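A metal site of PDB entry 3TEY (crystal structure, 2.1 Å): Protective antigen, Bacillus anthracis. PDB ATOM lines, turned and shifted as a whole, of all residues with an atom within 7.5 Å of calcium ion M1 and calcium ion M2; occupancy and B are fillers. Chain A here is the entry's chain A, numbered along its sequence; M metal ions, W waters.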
ATOM      1  N   PRO A 176     -22.950 -12.391  31.231  1.00  0.00           N
ATOM      2  CA  PRO A 176     -23.606 -12.445  29.919  1.00  0.00           C
ATOM      3  C   PRO A 176     -23.032 -11.366  28.982  1.00  0.00           C
ATOM      4  O   PRO A 176     -23.232 -10.173  29.210  1.00  0.00           O
ATOM      5  CB  PRO A 176     -25.072 -12.142  30.242  1.00  0.00           C
ATOM      6  CG  PRO A 176     -25.228 -12.513  31.712  1.00  0.00           C
ATOM      7  CD  PRO A 176     -23.910 -12.203  32.338  1.00  0.00           C
ATOM      8  N   ASP A 177     -22.280 -11.805  27.978  1.00  0.00           N
ATOM      9  CA  ASP A 177     -21.733 -10.942  26.943  1.00  0.00           C
ATOM     10  C   ASP A 177     -21.794 -11.716  25.633  1.00  0.00           C
ATOM     11  O   ASP A 177     -20.765 -12.121  25.089  1.00  0.00           O
ATOM     12  CB  ASP A 177     -20.293 -10.546  27.273  1.00  0.00           C
ATOM     13  CG  ASP A 177     -19.754  -9.494  26.323  1.00  0.00           C
ATOM     14  OD1 ASP A 177     -20.564  -8.834  25.663  1.00  0.00           O
ATOM     15  OD2 ASP A 177     -18.522  -9.322  26.221  1.00  0.00           O
ATOM     16  N   ARG A 178     -23.015 -11.912  25.128  1.00  0.00           N
ATOM     17  CA  ARG A 178     -23.247 -12.799  23.982  1.00  0.00           C
ATOM     18  C   ARG A 178     -22.418 -12.437  22.751  1.00  0.00           C
ATOM     19  O   ARG A 178     -21.965 -13.323  22.030  1.00  0.00           O
ATOM     20  CB  ARG A 178     -24.751 -12.895  23.628  1.00  0.00           C
ATOM     21  CG  ARG A 178     -25.629 -13.404  24.785  1.00  0.00           C
ATOM     22  CD  ARG A 178     -27.133 -13.143  24.564  1.00  0.00           C
ATOM     23  NE  ARG A 178     -27.754 -14.097  23.639  1.00  0.00           N
ATOM     24  CZ  ARG A 178     -28.166 -15.310  23.993  1.00  0.00           C
ATOM     25  NH1 ARG A 178     -28.027 -15.728  25.250  1.00  0.00           N
ATOM     26  NH2 ARG A 178     -28.726 -16.116  23.089  1.00  0.00           N
ATOM     27  N   ASP A 179     -22.193 -11.150  22.497  1.00  0.00           N
ATOM     28  CA  ASP A 179     -21.462 -10.760  21.290  1.00  0.00           C
ATOM     29  C   ASP A 179     -19.969 -10.525  21.538  1.00  0.00           C
ATOM     30  O   ASP A 179     -19.226 -10.154  20.623  1.00  0.00           O
ATOM     31  CB  ASP A 179     -22.089  -9.526  20.658  1.00  0.00           C
ATOM     32  CG  ASP A 179     -22.163  -8.365  21.619  1.00  0.00           C
ATOM     33  OD1 ASP A 179     -21.432  -8.373  22.619  1.00  0.00           O
ATOM     34  OD2 ASP A 179     -22.971  -7.455  21.394  1.00  0.00           O
ATOM     35  N   ASN A 180     -19.538 -10.709  22.785  1.00  0.00           N
ATOM     36  CA  ASN A 180     -18.124 -10.583  23.141  1.00  0.00           C
ATOM     37  C   ASN A 180     -17.527  -9.207  22.921  1.00  0.00           C
ATOM     38  O   ASN A 180     -16.328  -9.107  22.680  1.00  0.00           O
ATOM     39  CB  ASN A 180     -17.270 -11.620  22.404  1.00  0.00           C
ATOM     40  CG  ASN A 180     -15.960 -11.943  23.142  1.00  0.00           C
ATOM     41  OD1 ASN A 180     -15.960 -12.077  24.371  1.00  0.00           O
ATOM     42  ND2 ASN A 180     -14.867 -12.045  22.406  1.00  0.00           N
ATOM     43  N   ASP A 181     -18.331  -8.143  23.000  1.00  0.00           N
ATOM     44  CA  ASP A 181     -17.711  -6.810  22.852  1.00  0.00           C
ATOM     45  C   ASP A 181     -17.191  -6.256  24.179  1.00  0.00           C
ATOM     46  O   ASP A 181     -16.426  -5.291  24.186  1.00  0.00           O
ATOM     47  CB  ASP A 181     -18.592  -5.803  22.095  1.00  0.00           C
ATOM     48  CG  ASP A 181     -19.941  -5.594  22.743  1.00  0.00           C
ATOM     49  OD1 ASP A 181     -20.096  -5.851  23.960  1.00  0.00           O
ATOM     50  OD2 ASP A 181     -20.849  -5.117  22.013  1.00  0.00           O
ATOM     51  N   GLY A 182     -17.593  -6.875  25.292  1.00  0.00           N
ATOM     52  CA  GLY A 182     -17.152  -6.428  26.612  1.00  0.00           C
ATOM     53  C   GLY A 182     -18.225  -5.712  27.411  1.00  0.00           C
ATOM     54  O   GLY A 182     -18.119  -5.556  28.627  1.00  0.00           O
ATOM     55  N   ILE A 183     -19.280  -5.260  26.721  1.00  0.00           N
ATOM     56  CA  ILE A 183     -20.425  -4.684  27.429  1.00  0.00           C
ATOM     57  C   ILE A 183     -21.416  -5.800  27.798  1.00  0.00           C
ATOM     58  O   ILE A 183     -21.839  -6.575  26.957  1.00  0.00           O
ATOM     59  CB  ILE A 183     -21.140  -3.630  26.589  1.00  0.00           C
ATOM     60  CG1 ILE A 183     -20.121  -2.682  25.933  1.00  0.00           C
ATOM     61  CG2 ILE A 183     -22.112  -2.830  27.454  1.00  0.00           C
ATOM     62  CD1 ILE A 183     -20.770  -1.624  24.983  1.00  0.00           C
ATOM     63  N   PRO A 184     -21.777  -5.899  29.097  1.00  0.00           N
ATOM     64  CA  PRO A 184     -22.780  -6.885  29.496  1.00  0.00           C
ATOM     65  C   PRO A 184     -24.108  -6.741  28.755  1.00  0.00           C
ATOM     66  O   PRO A 184     -24.570  -5.610  28.518  1.00  0.00           O
ATOM     67  CB  PRO A 184     -22.982  -6.583  30.994  1.00  0.00           C
ATOM     68  CG  PRO A 184     -21.639  -6.100  31.448  1.00  0.00           C
ATOM     69  CD  PRO A 184     -21.045  -5.349  30.257  1.00  0.00           C
ATOM     70  N   ASP A 185     -24.710  -7.875  28.390  1.00  0.00           N
ATOM     71  CA  ASP A 185     -26.026  -7.889  27.767  1.00  0.00           C
ATOM     72  C   ASP A 185     -26.965  -6.859  28.372  1.00  0.00           C
ATOM     73  O   ASP A 185     -27.626  -6.099  27.657  1.00  0.00           O
ATOM     74  CB  ASP A 185     -26.699  -9.270  27.946  1.00  0.00           C
ATOM     75  CG  ASP A 185     -26.055 -10.383  27.131  1.00  0.00           C
ATOM     76  OD1 ASP A 185     -24.889 -10.249  26.689  1.00  0.00           O
ATOM     77  OD2 ASP A 185     -26.723 -11.436  26.942  1.00  0.00           O
ATOM     78  N   SER A 186     -27.060  -6.863  29.707  1.00  0.00           N
ATOM     79  CA  SER A 186     -28.075  -6.066  30.391  1.00  0.00           C
ATOM     80  C   SER A 186     -27.890  -4.558  30.195  1.00  0.00           C
ATOM     81  O   SER A 186     -28.867  -3.805  30.122  1.00  0.00           O
ATOM     82  CB  SER A 186     -28.162  -6.417  31.882  1.00  0.00           C
ATOM     83  OG  SER A 186     -26.951  -6.117  32.565  1.00  0.00           O
ATOM     84  N   GLU A 188     -26.313  -3.093  27.537  1.00  0.00           N
ATOM     85  CA  GLU A 188     -26.587  -2.752  26.148  1.00  0.00           C
ATOM     86  C   GLU A 188     -28.083  -2.583  25.929  1.00  0.00           C
ATOM     87  O   GLU A 188     -28.517  -1.707  25.180  1.00  0.00           O
ATOM     88  CB  GLU A 188     -26.031  -3.826  25.213  1.00  0.00           C
ATOM     89  CG  GLU A 188     -24.528  -3.895  25.254  1.00  0.00           C
ATOM     90  CD  GLU A 188     -23.965  -4.405  23.969  1.00  0.00           C
ATOM     91  OE1 GLU A 188     -24.020  -3.674  22.970  1.00  0.00           O
ATOM     92  OE2 GLU A 188     -23.480  -5.544  23.935  1.00  0.00           O
ATOM     93  N   TYR A 192     -26.828   2.660  28.815  1.00  0.00           N
ATOM     94  CA  TYR A 192     -25.616   2.923  29.567  1.00  0.00           C
ATOM     95  C   TYR A 192     -25.016   4.288  29.223  1.00  0.00           C
ATOM     96  O   TYR A 192     -25.433   4.942  28.261  1.00  0.00           O
ATOM     97  CB  TYR A 192     -24.590   1.804  29.363  1.00  0.00           C
ATOM     98  CG  TYR A 192     -24.192   1.535  27.912  1.00  0.00           C
ATOM     99  CD1 TYR A 192     -25.000   0.760  27.084  1.00  0.00           C
ATOM    100  CD2 TYR A 192     -23.015   2.036  27.386  1.00  0.00           C
ATOM    101  CE1 TYR A 192     -24.642   0.511  25.777  1.00  0.00           C
ATOM    102  CE2 TYR A 192     -22.651   1.784  26.064  1.00  0.00           C
ATOM    103  CZ  TYR A 192     -23.464   1.012  25.265  1.00  0.00           C
ATOM    104  OH  TYR A 192     -23.127   0.753  23.953  1.00  0.00           O
ATOM    105  N   SER A 221     -27.379  -0.466  22.519  1.00  0.00           N
ATOM    106  CA  SER A 221     -26.797  -1.184  21.381  1.00  0.00           C
ATOM    107  C   SER A 221     -27.276  -2.627  21.447  1.00  0.00           C
ATOM    108  O   SER A 221     -27.841  -3.040  22.462  1.00  0.00           O
ATOM    109  CB  SER A 221     -25.270  -1.094  21.407  1.00  0.00           C
ATOM    110  OG  SER A 221     -24.759  -1.293  22.720  1.00  0.00           O
ATOM    111  N   SER A 222     -27.087  -3.409  20.388  1.00  0.00           N
ATOM    112  CA  SER A 222     -27.553  -4.791  20.430  1.00  0.00           C
ATOM    113  C   SER A 222     -26.611  -5.651  21.265  1.00  0.00           C
ATOM    114  O   SER A 222     -25.404  -5.627  21.029  1.00  0.00           O
ATOM    115  CB  SER A 222     -27.663  -5.416  19.036  1.00  0.00           C
ATOM    116  OG  SER A 222     -27.863  -6.818  19.152  1.00  0.00           O
ATOM    117  N   PRO A 223     -27.163  -6.424  22.211  1.00  0.00           N
ATOM    118  CA  PRO A 223     -26.343  -7.370  22.997  1.00  0.00           C
ATOM    119  C   PRO A 223     -25.875  -8.520  22.138  1.00  0.00           C
ATOM    120  O   PRO A 223     -25.057  -9.333  22.601  1.00  0.00           O
ATOM    121  CB  PRO A 223     -27.322  -7.902  24.059  1.00  0.00           C
ATOM    122  CG  PRO A 223     -28.707  -7.813  23.356  1.00  0.00           C
ATOM    123  CD  PRO A 223     -28.593  -6.496  22.560  1.00  0.00           C
ATOM    124  N   GLU A 224     -26.373  -8.620  20.899  1.00  0.00           N
ATOM    125  CA  GLU A 224     -25.972  -9.721  20.027  1.00  0.00           C
ATOM    126  C   GLU A 224     -25.176  -9.335  18.789  1.00  0.00           C
ATOM    127  O   GLU A 224     -24.797 -10.194  17.989  1.00  0.00           O
ATOM    128  CB  GLU A 224     -27.181 -10.599  19.655  1.00  0.00           C
ATOM    129  CG  GLU A 224     -27.778 -11.278  20.883  1.00  0.00           C
ATOM    130  CD  GLU A 224     -28.934 -12.221  20.561  1.00  0.00           C
ATOM    131  OE1 GLU A 224     -28.967 -12.789  19.442  1.00  0.00           O
ATOM    132  OE2 GLU A 224     -29.805 -12.394  21.445  1.00  0.00           O
ATOM    133  N   LYS A 225     -24.894  -8.037  18.643  1.00  0.00           N
ATOM    134  CA  LYS A 225     -23.990  -7.573  17.585  1.00  0.00           C
ATOM    135  C   LYS A 225     -22.771  -6.842  18.141  1.00  0.00           C
ATOM    136  O   LYS A 225     -22.886  -5.790  18.765  1.00  0.00           O
ATOM    137  CB  LYS A 225     -24.706  -6.649  16.595  1.00  0.00           C
ATOM    138  CG  LYS A 225     -26.008  -7.197  16.027  1.00  0.00           C
ATOM    139  CD  LYS A 225     -26.563  -6.251  14.958  1.00  0.00           C
ATOM    140  CE  LYS A 225     -25.521  -5.991  13.887  1.00  0.00           C
ATOM    141  NZ  LYS A 225     -26.099  -5.237  12.772  1.00  0.00           N
ATOM    142  N   TRP A 226     -21.599  -7.403  17.847  1.00  0.00           N
ATOM    143  CA  TRP A 226     -20.332  -6.865  18.289  1.00  0.00           C
ATOM    144  C   TRP A 226     -20.190  -5.386  17.887  1.00  0.00           C
ATOM    145  O   TRP A 226     -19.778  -4.550  18.708  1.00  0.00           O
ATOM    146  CB  TRP A 226     -19.231  -7.733  17.663  1.00  0.00           C
ATOM    147  CG  TRP A 226     -17.843  -7.378  18.004  1.00  0.00           C
ATOM    148  CD1 TRP A 226     -17.159  -7.763  19.121  1.00  0.00           C
ATOM    149  CD2 TRP A 226     -16.927  -6.617  17.213  1.00  0.00           C
ATOM    150  NE1 TRP A 226     -15.877  -7.278  19.074  1.00  0.00           N
ATOM    151  CE2 TRP A 226     -15.708  -6.568  17.911  1.00  0.00           C
ATOM    152  CE3 TRP A 226     -17.026  -5.957  15.969  1.00  0.00           C
ATOM    153  CZ2 TRP A 226     -14.596  -5.889  17.421  1.00  0.00           C
ATOM    154  CZ3 TRP A 226     -15.912  -5.279  15.492  1.00  0.00           C
ATOM    155  CH2 TRP A 226     -14.713  -5.251  16.220  1.00  0.00           C
ATOM    156  N   SER A 227     -20.551  -5.069  16.637  1.00  0.00           N
ATOM    157  CA  SER A 227     -20.756  -3.687  16.175  1.00  0.00           C
ATOM    158  C   SER A 227     -22.237  -3.555  15.800  1.00  0.00           C
ATOM    159  O   SER A 227     -22.697  -4.146  14.811  1.00  0.00           O
ATOM    160  CB  SER A 227     -19.906  -3.350  14.946  1.00  0.00           C
ATOM    161  OG  SER A 227     -20.208  -2.046  14.411  1.00  0.00           O
ATOM    162  N   THR A 228     -22.984  -2.796  16.571  1.00  0.00           N
ATOM    163  CA  THR A 228     -24.409  -2.688  16.299  1.00  0.00           C
ATOM    164  C   THR A 228     -24.706  -2.085  14.912  1.00  0.00           C
ATOM    165  O   THR A 228     -25.717  -2.425  14.296  1.00  0.00           O
ATOM    166  CB  THR A 228     -25.144  -1.973  17.437  1.00  0.00           C
ATOM    167  OG1 THR A 228     -25.017  -2.767  18.627  1.00  0.00           O
ATOM    168  CG2 THR A 228     -26.639  -1.770  17.107  1.00  0.00           C
ATOM    169  N   SER A 234     -16.127  -2.165  17.357  1.00  0.00           N
ATOM    170  CA  SER A 234     -17.126  -2.717  18.276  1.00  0.00           C
ATOM    171  C   SER A 234     -17.832  -1.631  19.069  1.00  0.00           C
ATOM    172  O   SER A 234     -17.346  -0.507  19.226  1.00  0.00           O
ATOM    173  CB  SER A 234     -16.486  -3.726  19.254  1.00  0.00           C
ATOM    174  OG  SER A 234     -16.063  -3.074  20.441  1.00  0.00           O
ATOM    175  N   ASP A 235     -18.987  -1.990  19.621  1.00  0.00           N
ATOM    176  CA  ASP A 235     -19.721  -1.040  20.446  1.00  0.00           C
ATOM    177  C   ASP A 235     -18.870  -0.533  21.606  1.00  0.00           C
ATOM    178  O   ASP A 235     -18.928   0.653  21.993  1.00  0.00           O
ATOM    179  CB  ASP A 235     -21.009  -1.705  20.942  1.00  0.00           C
ATOM    180  CG  ASP A 235     -21.952  -2.119  19.799  1.00  0.00           C
ATOM    181  OD1 ASP A 235     -21.908  -1.511  18.686  1.00  0.00           O
ATOM    182  OD2 ASP A 235     -22.757  -3.047  20.053  1.00  0.00           O
ATOM    183  N   PHE A 236     -18.094  -1.446  22.201  1.00  0.00           N
ATOM    184  CA  PHE A 236     -17.170  -1.131  23.301  1.00  0.00           C
ATOM    185  C   PHE A 236     -15.984  -0.262  22.863  1.00  0.00           C
ATOM    186  O   PHE A 236     -15.631   0.730  23.529  1.00  0.00           O
ATOM    187  CB  PHE A 236     -16.685  -2.437  23.932  1.00  0.00           C
ATOM    188  CG  PHE A 236     -15.789  -2.269  25.099  1.00  0.00           C
ATOM    189  CD1 PHE A 236     -16.313  -1.917  26.341  1.00  0.00           C
ATOM    190  CD2 PHE A 236     -14.439  -2.523  24.999  1.00  0.00           C
ATOM    191  CE1 PHE A 236     -15.485  -1.795  27.463  1.00  0.00           C
ATOM    192  CE2 PHE A 236     -13.604  -2.406  26.120  1.00  0.00           C
ATOM    193  CZ  PHE A 236     -14.138  -2.047  27.349  1.00  0.00           C
ATOM    194  N   PRO A 254     -22.546   3.940  19.095  1.00  0.00           N
ATOM    195  CA  PRO A 254     -22.718   2.572  18.607  1.00  0.00           C
ATOM    196  C   PRO A 254     -23.836   2.424  17.560  1.00  0.00           C
ATOM    197  O   PRO A 254     -23.880   1.400  16.861  1.00  0.00           O
ATOM    198  CB  PRO A 254     -23.110   1.797  19.881  1.00  0.00           C
ATOM    199  CG  PRO A 254     -22.631   2.626  21.028  1.00  0.00           C
ATOM    200  CD  PRO A 254     -22.721   4.065  20.556  1.00  0.00           C
HETATM  201 CA    CA M   1     -21.954  -7.229  24.670  1.00  0.00          CA
HETATM  202 CA    CA M   2     -23.026  -5.134  21.198  1.00  0.00          CA
HETATM  203  O   HOH W   1     -24.093  -8.779  24.907  1.00  0.00           O
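The backbone NH (N) of Asp 235 lies within hydrogen-bond range of the backbone carbonyl oxygen (O) of Trp 226, at 2.8 Å. The backbone NH (N) of Ser 222 lies within hydrogen-bond range of the side-chain hydroxyl (OG1) of Thr 228 (2.8 Å). OG of Ser 222 lies within hydrogen-bond range of N of Glu 224, 2.9 Å away. O of Thr 228 is in hydrogen-bond range of NZ of Lys 225, 3.2 Å away. The backbone NH (N) of Asp 179 lies close to the backbone carbonyl oxygen (O) of Pro 223 (3.4 Å). The backbone carbonyl oxygen (O) of Glu 188 sits at hydrogen-bond distance from the backbone NH (N) of Ser 221 (3.1 Å). The backbone NH (N) of Thr 228 sits at hydrogen-bond distance from the side-chain carboxylate (OD1) of Asp 235, at 2.7 Å. N of Lys 225 lies within hydrogen-bond range of OG of Ser 222 (3.2 Å).
Along chain A the residues within 4 Å of calcium ion M1 span positions 177 to 188.
The nearest printed residue that does not touch calcium ion M2 is Thr 228 (4.02 Å).
Calcium ion M1 is bound by OD1 of Asp 177 (2.3 Å), O of Ile 183 (2.4 Å), OE2 of Glu 188 (2.4 Å), OD1 of Asp 179 (2.4 Å), OD1 of Asp 181 (2.4 Å) and water W1 (2.7 Å). Calcium ion M1 has six donor atoms within binding distance.
Calcium ion M2 is bound by the side-chain carboxylate (OD2) of Asp 181 (2.3 Å), the side-chain carboxylate (OD2) of Asp 179 (2.3 Å), the side-chain carboxylate (OD2) of Asp 235 (2.4 Å), the backbone carbonyl oxygen (O) of Ser 222 (2.4 Å), the side-chain carboxylate (OE1) of Glu 188 (2.5 Å), the backbone carbonyl oxygen (O) of Lys 225 (2.5 Å) and the side-chain carboxylate (OE2) of Glu 188 (2.8 Å). Calcium ion M2 has seven donor atoms within binding distance.
Water W1 lies within hydrogen-bond range of OD1 of Asp 185 (2.4 Å), O of Pro 223 (2.6 Å) and N of Arg 178 (3.3 Å).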
